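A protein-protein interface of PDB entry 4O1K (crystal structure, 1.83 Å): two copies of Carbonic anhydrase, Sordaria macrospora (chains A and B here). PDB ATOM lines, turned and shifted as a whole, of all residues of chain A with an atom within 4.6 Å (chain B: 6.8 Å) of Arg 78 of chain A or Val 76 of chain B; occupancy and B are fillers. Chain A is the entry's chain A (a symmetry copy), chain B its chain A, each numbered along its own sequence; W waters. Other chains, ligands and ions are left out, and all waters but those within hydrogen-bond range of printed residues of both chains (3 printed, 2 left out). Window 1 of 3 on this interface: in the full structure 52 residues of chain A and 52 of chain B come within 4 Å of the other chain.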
ATOM      1  N   GLY A  55     -36.607 -28.703  17.777  1.00  0.00           N
ATOM      2  CA  GLY A  55     -35.996 -28.743  19.102  1.00  0.00           C
ATOM      3  C   GLY A  55     -34.966 -27.653  19.290  1.00  0.00           C
ATOM      4  O   GLY A  55     -34.774 -26.808  18.412  1.00  0.00           O
ATOM      5  N   CYS A  56     -34.289 -27.652  20.434  1.00  0.00           N
ATOM      6  CA  CYS A  56     -33.343 -26.555  20.717  1.00  0.00           C
ATOM      7  C   CYS A  56     -31.888 -26.915  20.417  1.00  0.00           C
ATOM      8  O   CYS A  56     -31.451 -28.063  20.636  1.00  0.00           O
ATOM      9  CB  CYS A  56     -33.498 -26.083  22.152  1.00  0.00           C
ATOM     10  SG  CYS A  56     -32.351 -24.720  22.555  1.00  0.00           S
ATOM     11  N   SER A  57     -31.131 -25.938  19.923  1.00  0.00           N
ATOM     12  CA  SER A  57     -29.735 -26.151  19.582  1.00  0.00           C
ATOM     13  C   SER A  57     -28.878 -26.505  20.804  1.00  0.00           C
ATOM     14  O   SER A  57     -27.810 -27.093  20.647  1.00  0.00           O
ATOM     15  CB  SER A  57     -29.168 -24.920  18.903  1.00  0.00           C
ATOM     16  OG  SER A  57     -29.777 -24.748  17.630  1.00  0.00           O
ATOM     17  N   SER A  59     -29.954 -28.186  23.556  1.00  0.00           N
ATOM     18  CA  SER A  59     -30.334 -29.443  24.189  1.00  0.00           C
ATOM     19  C   SER A  59     -29.187 -30.412  23.895  1.00  0.00           C
ATOM     20  O   SER A  59     -28.450 -30.217  22.933  1.00  0.00           O
ATOM     21  CB  SER A  59     -31.661 -29.950  23.625  1.00  0.00           C
ATOM     22  OG  SER A  59     -31.556 -30.283  22.248  1.00  0.00           O
ATOM     23  N   PRO A  62     -29.792 -36.017  21.217  1.00  0.00           N
ATOM     24  CA  PRO A  62     -30.569 -36.015  19.969  1.00  0.00           C
ATOM     25  C   PRO A  62     -31.961 -36.618  20.171  1.00  0.00           C
ATOM     26  O   PRO A  62     -32.112 -37.543  20.969  1.00  0.00           O
ATOM     27  CB  PRO A  62     -29.749 -36.925  19.041  1.00  0.00           C
ATOM     28  CG  PRO A  62     -28.395 -36.958  19.626  1.00  0.00           C
ATOM     29  CD  PRO A  62     -28.565 -36.819  21.102  1.00  0.00           C
ATOM     30  N   VAL A  76     -35.510 -33.132  11.318  1.00  0.00           N
ATOM     31  CA  VAL A  76     -35.191 -32.354  12.517  1.00  0.00           C
ATOM     32  C   VAL A  76     -34.766 -30.908  12.209  1.00  0.00           C
ATOM     33  O   VAL A  76     -33.888 -30.669  11.367  1.00  0.00           O
ATOM     34  CB  VAL A  76     -34.045 -33.048  13.315  1.00  0.00           C
ATOM     35  CG1 VAL A  76     -33.592 -32.204  14.502  1.00  0.00           C
ATOM     36  CG2 VAL A  76     -34.491 -34.397  13.824  1.00  0.00           C
ATOM     37  N   HIS A  77     -35.411 -29.962  12.870  1.00  0.00           N
ATOM     38  CA  HIS A  77     -34.951 -28.575  12.872  1.00  0.00           C
ATOM     39  C   HIS A  77     -34.538 -28.252  14.300  1.00  0.00           C
ATOM     40  O   HIS A  77     -35.268 -28.537  15.216  1.00  0.00           O
ATOM     41  CB  HIS A  77     -36.060 -27.620  12.400  1.00  0.00           C
ATOM     42  CG  HIS A  77     -35.692 -26.175  12.535  1.00  0.00           C
ATOM     43  ND1 HIS A  77     -34.825 -25.548  11.668  1.00  0.00           N
ATOM     44  CD2 HIS A  77     -36.047 -25.241  13.448  1.00  0.00           C
ATOM     45  CE1 HIS A  77     -34.659 -24.289  12.038  1.00  0.00           C
ATOM     46  NE2 HIS A  77     -35.385 -24.079  13.118  1.00  0.00           N
ATOM     47  N   ARG A  78     -33.368 -27.648  14.489  1.00  0.00           N
ATOM     48  CA  ARG A  78     -32.986 -27.233  15.839  1.00  0.00           C
ATOM     49  C   ARG A  78     -32.507 -25.806  15.784  1.00  0.00           C
ATOM     50  O   ARG A  78     -31.669 -25.463  14.915  1.00  0.00           O
ATOM     51  CB  ARG A  78     -31.862 -28.132  16.390  1.00  0.00           C
ATOM     52  CG  ARG A  78     -32.398 -29.400  17.033  1.00  0.00           C
ATOM     53  CD  ARG A  78     -31.300 -30.434  17.346  1.00  0.00           C
ATOM     54  NE  ARG A  78     -30.544 -30.092  18.547  1.00  0.00           N
ATOM     55  CZ  ARG A  78     -29.558 -30.853  19.037  1.00  0.00           C
ATOM     56  NH1 ARG A  78     -29.240 -31.988  18.424  1.00  0.00           N
ATOM     57  NH2 ARG A  78     -28.898 -30.496  20.137  1.00  0.00           N
ATOM     58  N   ASN A  79     -33.034 -24.979  16.691  1.00  0.00           N
ATOM     59  CA  ASN A  79     -32.617 -23.562  16.725  1.00  0.00           C
ATOM     60  C   ASN A  79     -32.562 -23.102  18.165  1.00  0.00           C
ATOM     61  O   ASN A  79     -32.910 -23.866  19.040  1.00  0.00           O
ATOM     62  CB  ASN A  79     -33.543 -22.668  15.883  1.00  0.00           C
ATOM     63  CG  ASN A  79     -34.954 -22.603  16.405  1.00  0.00           C
ATOM     64  OD1 ASN A  79     -35.198 -22.442  17.595  1.00  0.00           O
ATOM     65  ND2 ASN A  79     -35.921 -22.665  15.480  1.00  0.00           N
ATOM     66  N   TYR B  51     -18.018 -27.627  19.806  1.00  0.00           N
ATOM     67  CA  TYR B  51     -18.423 -27.551  18.388  1.00  0.00           C
ATOM     68  C   TYR B  51     -19.739 -26.847  18.203  1.00  0.00           C
ATOM     69  O   TYR B  51     -20.667 -27.063  18.992  1.00  0.00           O
ATOM     70  CB  TYR B  51     -18.659 -28.965  17.839  1.00  0.00           C
ATOM     71  CG  TYR B  51     -17.411 -29.787  17.588  1.00  0.00           C
ATOM     72  CD1 TYR B  51     -16.881 -29.891  16.307  1.00  0.00           C
ATOM     73  CD2 TYR B  51     -16.790 -30.488  18.616  1.00  0.00           C
ATOM     74  CE1 TYR B  51     -15.754 -30.641  16.065  1.00  0.00           C
ATOM     75  CE2 TYR B  51     -15.673 -31.245  18.377  1.00  0.00           C
ATOM     76  CZ  TYR B  51     -15.163 -31.314  17.101  1.00  0.00           C
ATOM     77  OH  TYR B  51     -14.042 -32.068  16.862  1.00  0.00           O
ATOM     78  N   LEU B  52     -19.824 -26.054  17.129  1.00  0.00           N
ATOM     79  CA  LEU B  52     -21.084 -25.686  16.490  1.00  0.00           C
ATOM     80  C   LEU B  52     -21.224 -26.559  15.235  1.00  0.00           C
ATOM     81  O   LEU B  52     -20.337 -26.595  14.393  1.00  0.00           O
ATOM     82  CB  LEU B  52     -21.082 -24.209  16.070  1.00  0.00           C
ATOM     83  CG  LEU B  52     -22.223 -23.788  15.140  1.00  0.00           C
ATOM     84  CD1 LEU B  52     -23.601 -24.022  15.780  1.00  0.00           C
ATOM     85  CD2 LEU B  52     -22.094 -22.326  14.705  1.00  0.00           C
ATOM     86  N   TRP B  53     -22.319 -27.294  15.135  1.00  0.00           N
ATOM     87  CA  TRP B  53     -22.542 -28.199  14.014  1.00  0.00           C
ATOM     88  C   TRP B  53     -23.715 -27.657  13.235  1.00  0.00           C
ATOM     89  O   TRP B  53     -24.809 -27.503  13.785  1.00  0.00           O
ATOM     90  CB  TRP B  53     -22.915 -29.573  14.556  1.00  0.00           C
ATOM     91  CG  TRP B  53     -23.111 -30.622  13.521  1.00  0.00           C
ATOM     92  CD1 TRP B  53     -24.230 -30.863  12.769  1.00  0.00           C
ATOM     93  CD2 TRP B  53     -22.151 -31.617  13.156  1.00  0.00           C
ATOM     94  NE1 TRP B  53     -23.998 -31.958  11.929  1.00  0.00           N
ATOM     95  CE2 TRP B  53     -22.727 -32.421  12.150  1.00  0.00           C
ATOM     96  CE3 TRP B  53     -20.846 -31.897  13.580  1.00  0.00           C
ATOM     97  CZ2 TRP B  53     -22.038 -33.499  11.570  1.00  0.00           C
ATOM     98  CZ3 TRP B  53     -20.170 -32.954  12.997  1.00  0.00           C
ATOM     99  CH2 TRP B  53     -20.765 -33.741  12.014  1.00  0.00           C
ATOM    100  N   ILE B  54     -23.507 -27.390  11.955  1.00  0.00           N
ATOM    101  CA  ILE B  54     -24.592 -26.943  11.074  1.00  0.00           C
ATOM    102  C   ILE B  54     -24.850 -28.062  10.079  1.00  0.00           C
ATOM    103  O   ILE B  54     -24.023 -28.333   9.200  1.00  0.00           O
ATOM    104  CB  ILE B  54     -24.208 -25.654  10.312  1.00  0.00           C
ATOM    105  CG1 ILE B  54     -23.852 -24.563  11.330  1.00  0.00           C
ATOM    106  CG2 ILE B  54     -25.385 -25.182   9.428  1.00  0.00           C
ATOM    107  CD1 ILE B  54     -23.314 -23.256  10.698  1.00  0.00           C
ATOM    108  N   GLY B  55     -25.978 -28.745  10.237  1.00  0.00           N
ATOM    109  CA  GLY B  55     -26.245 -29.912   9.402  1.00  0.00           C
ATOM    110  C   GLY B  55     -27.604 -29.845   8.744  1.00  0.00           C
ATOM    111  O   GLY B  55     -28.320 -28.849   8.874  1.00  0.00           O
ATOM    112  N   SER B  57     -31.607 -30.972   7.872  1.00  0.00           N
ATOM    113  CA  SER B  57     -32.788 -31.515   8.520  1.00  0.00           C
ATOM    114  C   SER B  57     -33.145 -32.917   8.012  1.00  0.00           C
ATOM    115  O   SER B  57     -33.835 -33.658   8.709  1.00  0.00           O
ATOM    116  CB  SER B  57     -33.969 -30.586   8.321  1.00  0.00           C
ATOM    117  OG  SER B  57     -33.754 -29.374   9.032  1.00  0.00           O
ATOM    118  N   PRO B  62     -27.931 -38.525  13.744  1.00  0.00           N
ATOM    119  CA  PRO B  62     -27.487 -37.355  14.516  1.00  0.00           C
ATOM    120  C   PRO B  62     -25.964 -37.216  14.503  1.00  0.00           C
ATOM    121  O   PRO B  62     -25.262 -38.228  14.492  1.00  0.00           O
ATOM    122  CB  PRO B  62     -27.958 -37.675  15.943  1.00  0.00           C
ATOM    123  CG  PRO B  62     -29.012 -38.694  15.787  1.00  0.00           C
ATOM    124  CD  PRO B  62     -28.655 -39.495  14.579  1.00  0.00           C
ATOM    125  N   ALA B  63     -25.476 -35.977  14.511  1.00  0.00           N
ATOM    126  CA  ALA B  63     -24.043 -35.681  14.522  1.00  0.00           C
ATOM    127  C   ALA B  63     -23.292 -36.427  15.610  1.00  0.00           C
ATOM    128  O   ALA B  63     -22.147 -36.869  15.417  1.00  0.00           O
ATOM    129  CB  ALA B  63     -23.842 -34.192  14.713  1.00  0.00           C
ATOM    130  N   GLU B  64     -23.949 -36.528  16.760  1.00  0.00           N
ATOM    131  CA  GLU B  64     -23.378 -37.114  17.961  1.00  0.00           C
ATOM    132  C   GLU B  64     -23.067 -38.586  17.727  1.00  0.00           C
ATOM    133  O   GLU B  64     -22.075 -39.120  18.231  1.00  0.00           O
ATOM    134  CB  GLU B  64     -24.356 -36.929  19.130  1.00  0.00           C
ATOM    135  CG  GLU B  64     -24.430 -35.483  19.693  1.00  0.00           C
ATOM    136  CD  GLU B  64     -25.610 -34.660  19.175  1.00  0.00           C
ATOM    137  OE1 GLU B  64     -26.113 -33.790  19.933  1.00  0.00           O
ATOM    138  OE2 GLU B  64     -26.030 -34.862  18.010  1.00  0.00           O
ATOM    139  N   ALA B  74     -21.665 -30.859  21.285  1.00  0.00           N
ATOM    140  CA  ALA B  74     -22.087 -30.187  20.059  1.00  0.00           C
ATOM    141  C   ALA B  74     -23.328 -29.353  20.285  1.00  0.00           C
ATOM    142  O   ALA B  74     -24.333 -29.778  20.883  1.00  0.00           O
ATOM    143  CB  ALA B  74     -22.319 -31.186  18.927  1.00  0.00           C
ATOM    144  N   PHE B  75     -23.238 -28.134  19.810  1.00  0.00           N
ATOM    145  CA  PHE B  75     -24.365 -27.244  19.748  1.00  0.00           C
ATOM    146  C   PHE B  75     -24.828 -27.399  18.321  1.00  0.00           C
ATOM    147  O   PHE B  75     -24.020 -27.221  17.429  1.00  0.00           O
ATOM    148  CB  PHE B  75     -23.790 -25.868  19.936  1.00  0.00           C
ATOM    149  CG  PHE B  75     -24.789 -24.846  20.208  1.00  0.00           C
ATOM    150  CD1 PHE B  75     -25.429 -24.807  21.431  1.00  0.00           C
ATOM    151  CD2 PHE B  75     -25.078 -23.889  19.262  1.00  0.00           C
ATOM    152  CE1 PHE B  75     -26.369 -23.834  21.689  1.00  0.00           C
ATOM    153  CE2 PHE B  75     -26.010 -22.916  19.531  1.00  0.00           C
ATOM    154  CZ  PHE B  75     -26.661 -22.890  20.737  1.00  0.00           C
ATOM    155  N   VAL B  76     -26.108 -27.712  18.076  1.00  0.00           N
ATOM    156  CA  VAL B  76     -26.519 -28.169  16.747  1.00  0.00           C
ATOM    157  C   VAL B  76     -27.606 -27.287  16.108  1.00  0.00           C
ATOM    158  O   VAL B  76     -28.635 -26.994  16.734  1.00  0.00           O
ATOM    159  CB  VAL B  76     -27.052 -29.633  16.825  1.00  0.00           C
ATOM    160  CG1 VAL B  76     -27.611 -30.103  15.487  1.00  0.00           C
ATOM    161  CG2 VAL B  76     -25.953 -30.577  17.249  1.00  0.00           C
ATOM    162  N   HIS B  77     -27.354 -26.852  14.885  1.00  0.00           N
ATOM    163  CA  HIS B  77     -28.387 -26.224  14.065  1.00  0.00           C
ATOM    164  C   HIS B  77     -28.629 -27.148  12.881  1.00  0.00           C
ATOM    165  O   HIS B  77     -27.694 -27.585  12.258  1.00  0.00           O
ATOM    166  CB  HIS B  77     -27.945 -24.831  13.583  1.00  0.00           C
ATOM    167  CG  HIS B  77     -28.900 -24.213  12.610  1.00  0.00           C
ATOM    168  ND1 HIS B  77     -30.101 -23.664  12.999  1.00  0.00           N
ATOM    169  CD2 HIS B  77     -28.848 -24.081  11.264  1.00  0.00           C
ATOM    170  CE1 HIS B  77     -30.752 -23.220  11.936  1.00  0.00           C
ATOM    171  NE2 HIS B  77     -30.015 -23.466  10.870  1.00  0.00           N
ATOM    172  N   ARG B  78     -29.888 -27.440  12.565  1.00  0.00           N
ATOM    173  CA  ARG B  78     -30.159 -28.244  11.374  1.00  0.00           C
ATOM    174  C   ARG B  78     -31.238 -27.564  10.572  1.00  0.00           C
ATOM    175  O   ARG B  78     -32.284 -27.172  11.142  1.00  0.00           O
ATOM    176  CB  ARG B  78     -30.624 -29.660  11.764  1.00  0.00           C
ATOM    177  CG  ARG B  78     -29.460 -30.603  12.019  1.00  0.00           C
ATOM    178  CD  ARG B  78     -29.886 -31.934  12.667  1.00  0.00           C
ATOM    179  NE  ARG B  78     -30.477 -32.855  11.702  1.00  0.00           N
ATOM    180  CZ  ARG B  78     -30.896 -34.085  12.021  1.00  0.00           C
ATOM    181  NH1 ARG B  78     -30.769 -34.517  13.271  1.00  0.00           N
ATOM    182  NH2 ARG B  78     -31.430 -34.888  11.103  1.00  0.00           N
ATOM    183  N   ASN B  79     -30.987 -27.414   9.269  1.00  0.00           N
ATOM    184  CA  ASN B  79     -31.991 -26.769   8.396  1.00  0.00           C
ATOM    185  C   ASN B  79     -31.982 -27.455   7.048  1.00  0.00           C
ATOM    186  O   ASN B  79     -31.168 -28.330   6.840  1.00  0.00           O
ATOM    187  CB  ASN B  79     -31.750 -25.256   8.260  1.00  0.00           C
ATOM    188  CG  ASN B  79     -30.455 -24.913   7.572  1.00  0.00           C
ATOM    189  OD1 ASN B  79     -30.095 -25.481   6.547  1.00  0.00           O
ATOM    190  ND2 ASN B  79     -29.756 -23.907   8.113  1.00  0.00           N
ATOM    191  N   ASN B  90     -31.989 -16.785  12.130  1.00  0.00           N
ATOM    192  CA  ASN B  90     -31.960 -18.046  12.860  1.00  0.00           C
ATOM    193  C   ASN B  90     -30.479 -18.512  12.949  1.00  0.00           C
ATOM    194  O   ASN B  90     -29.855 -18.526  14.058  1.00  0.00           O
ATOM    195  CB  ASN B  90     -32.883 -19.010  12.107  1.00  0.00           C
ATOM    196  CG  ASN B  90     -33.115 -20.297  12.842  1.00  0.00           C
ATOM    197  OD1 ASN B  90     -32.254 -20.744  13.605  1.00  0.00           O
ATOM    198  ND2 ASN B  90     -34.277 -20.912  12.616  1.00  0.00           N
ATOM    199  N   VAL B  94     -27.396 -18.012  15.736  1.00  0.00           N
ATOM    200  CA  VAL B  94     -26.686 -19.132  16.349  1.00  0.00           C
ATOM    201  C   VAL B  94     -25.133 -19.149  16.161  1.00  0.00           C
ATOM    202  O   VAL B  94     -24.394 -19.564  17.073  1.00  0.00           O
ATOM    203  CB  VAL B  94     -27.341 -20.457  16.053  1.00  0.00           C
ATOM    204  CG1 VAL B  94     -27.026 -20.924  14.686  1.00  0.00           C
ATOM    205  CG2 VAL B  94     -26.823 -21.440  17.005  1.00  0.00           C
HETATM  206  O   HOH W   1     -29.297 -22.865  16.051  1.00  0.00           O
HETATM  207  O   HOH W   2     -25.454 -29.462  23.140  1.00  0.00           O
HETATM  208  O   HOH W   3     -35.324 -27.423   9.052  1.00  0.00           O
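The side-chain hydroxyl (OG) of Ser 57 of chain B lies within hydrogen-bond range of the backbone carbonyl oxygen (O) of Val 76 of chain A (2.7 Å).
The guanidinium group (NH1) of Arg 78 of chain A lies within salt-bridge range of the side-chain carboxylate (OE1) of Glu 64 of chain B (3.9 Å).
O of Val 76 of chain B is in hydrogen-bond range of OG of Ser 57 of chain A (2.7 Å).
A ring nitrogen (ND1) of His 77 of chain B sits at hydrogen-bond distance from the backbone carbonyl oxygen of Arg 78 of chain A (3.1 Å).
A ring nitrogen (ND1) of His 77 of chain A sits at hydrogen-bond distance from the backbone carbonyl oxygen (O) of Arg 78 of chain B (3.1 Å).
The side-chain amide nitrogen of Asn 90 of chain B is in hydrogen-bond range of a ring nitrogen (NE2) of His 77 of chain A, at 3.4 Å.
O of Tyr 51 of chain B sits at hydrogen-bond distance from N of Phe 75 of chain B, 2.9 Å away.
The backbone carbonyl oxygen of Arg 78 of chain B lies within hydrogen-bond range of the side-chain hydroxyl of Ser 57 of chain B.
The backbone carbonyl oxygen (O) of Gly 55 of chain A is in hydrogen-bond range of the backbone NH (N) of Asn 79 of chain A (3.1 Å).
O of Cys 56 of chain A sits at hydrogen-bond distance from NE of Arg 78 of chain A (3.1 Å).
O of Arg 78 of chain A lies within hydrogen-bond range of OG of Ser 57 of chain A.
The backbone carbonyl oxygen (O) of Ser 59 of chain A lies within hydrogen-bond range of the guanidinium group (NH2) of Arg 78 of chain A (2.8 Å).
Ser 57 of chain A touches Phe 75 of chain B (O to CD1, 3.4 Å).
Pro 62 of chain A touches Pro 62 of chain B.
Pro 62 of chain A touches Glu 64 of chain B.
CB of Arg 78 of chain B touches O of Val 76 of chain A (3.4 Å).
O of Val 76 of chain B touches CB of Arg 78 of chain A, 3.4 Å away.
Arg 78 of chain A touches Arg 78 of chain B (O to N, 3.6 Å).
Asn 90 of chain B touches Asn 79 of chain A.
Of the printed residues of chain B, His 77 of chain A touches Arg 78 (3.1 Å) and Asn 90 (3.4 Å).
Of chain B, only Glu 64 (3.9 Å), Val 76 (3.4 Å), His 77 (3.1 Å) and Arg 78 (3.6 Å) come within 4 Å of Arg 78 of chain A.
Trp 53 of chain B touches none of the printed residues of chain A.
Ala 74 of chain B touches none of the printed residues of chain A.
Of chain A, only Ser 57 and Arg 78 come within 4 Å of Val 76 of chain B.
Printed residues of chain A within 4 Å of His 77 of chain B: Arg 78 (3.1 Å).
The nearest residue of chain B that does not touch Arg 78 of chain A is Ala 74 of chain B (4.7 Å).
The nearest printed residue of chain A that does not touch Val 76 of chain B is Asn 79 of chain A (4.8 Å).
The nearest printed residue of chain A that does not touch Phe 75 of chain B is Arg 78 of chain A (5.4 Å).
Of the 9 printed residues of chain A, 6 touch a printed residue of chain B.
Hydrophobic or aromatic side chains of chain A that line the printed part of chain B: Pro 62, Val 76 and His 77.
Along chain A the printed residues that touch a printed residue of chain B span positions 57 to 79.
Of the 17 printed residues of chain B, 8 touch a printed residue of chain A.
Among the printed residues, Asp or Glu carboxylates within 4 Å of a Lys or Arg side-chain nitrogen of the other chain: Arg 78 of chain A with Glu 64 of chain B (3.9 Å).
Pro 62 of chain A touches its own counterpart, Pro 62 of chain B.
Val 76 of chain A touches Arg 78 of chain B, and with the chains exchanged Arg 78 of chain A touches Val 76 of chain B.
His 77 of chain A touches Arg 78 of chain B, and with the chains exchanged Arg 78 of chain A touches His 77 of chain B.
Arg 78 of chain A touches its own counterpart, Arg 78 of chain B.
Of the 13 pairs that touch across the chains among the printed residues, 8 have their exchanged pair printed and touching as well.
Water W3 bridges the side-chain hydroxyl (OG) of Ser 57 of chain B (2.5 Å) and a ring nitrogen (ND1) of His 77 of chain A (3.3 Å).
Water W1 bridges the side-chain hydroxyl of Ser 57 of chain A (2.5 Å) and a ring nitrogen (ND1) of His 77 of chain B (3.3 Å).
Water W2 bridges O of Ala 74 of chain B and O of Ser 59 of chain A.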
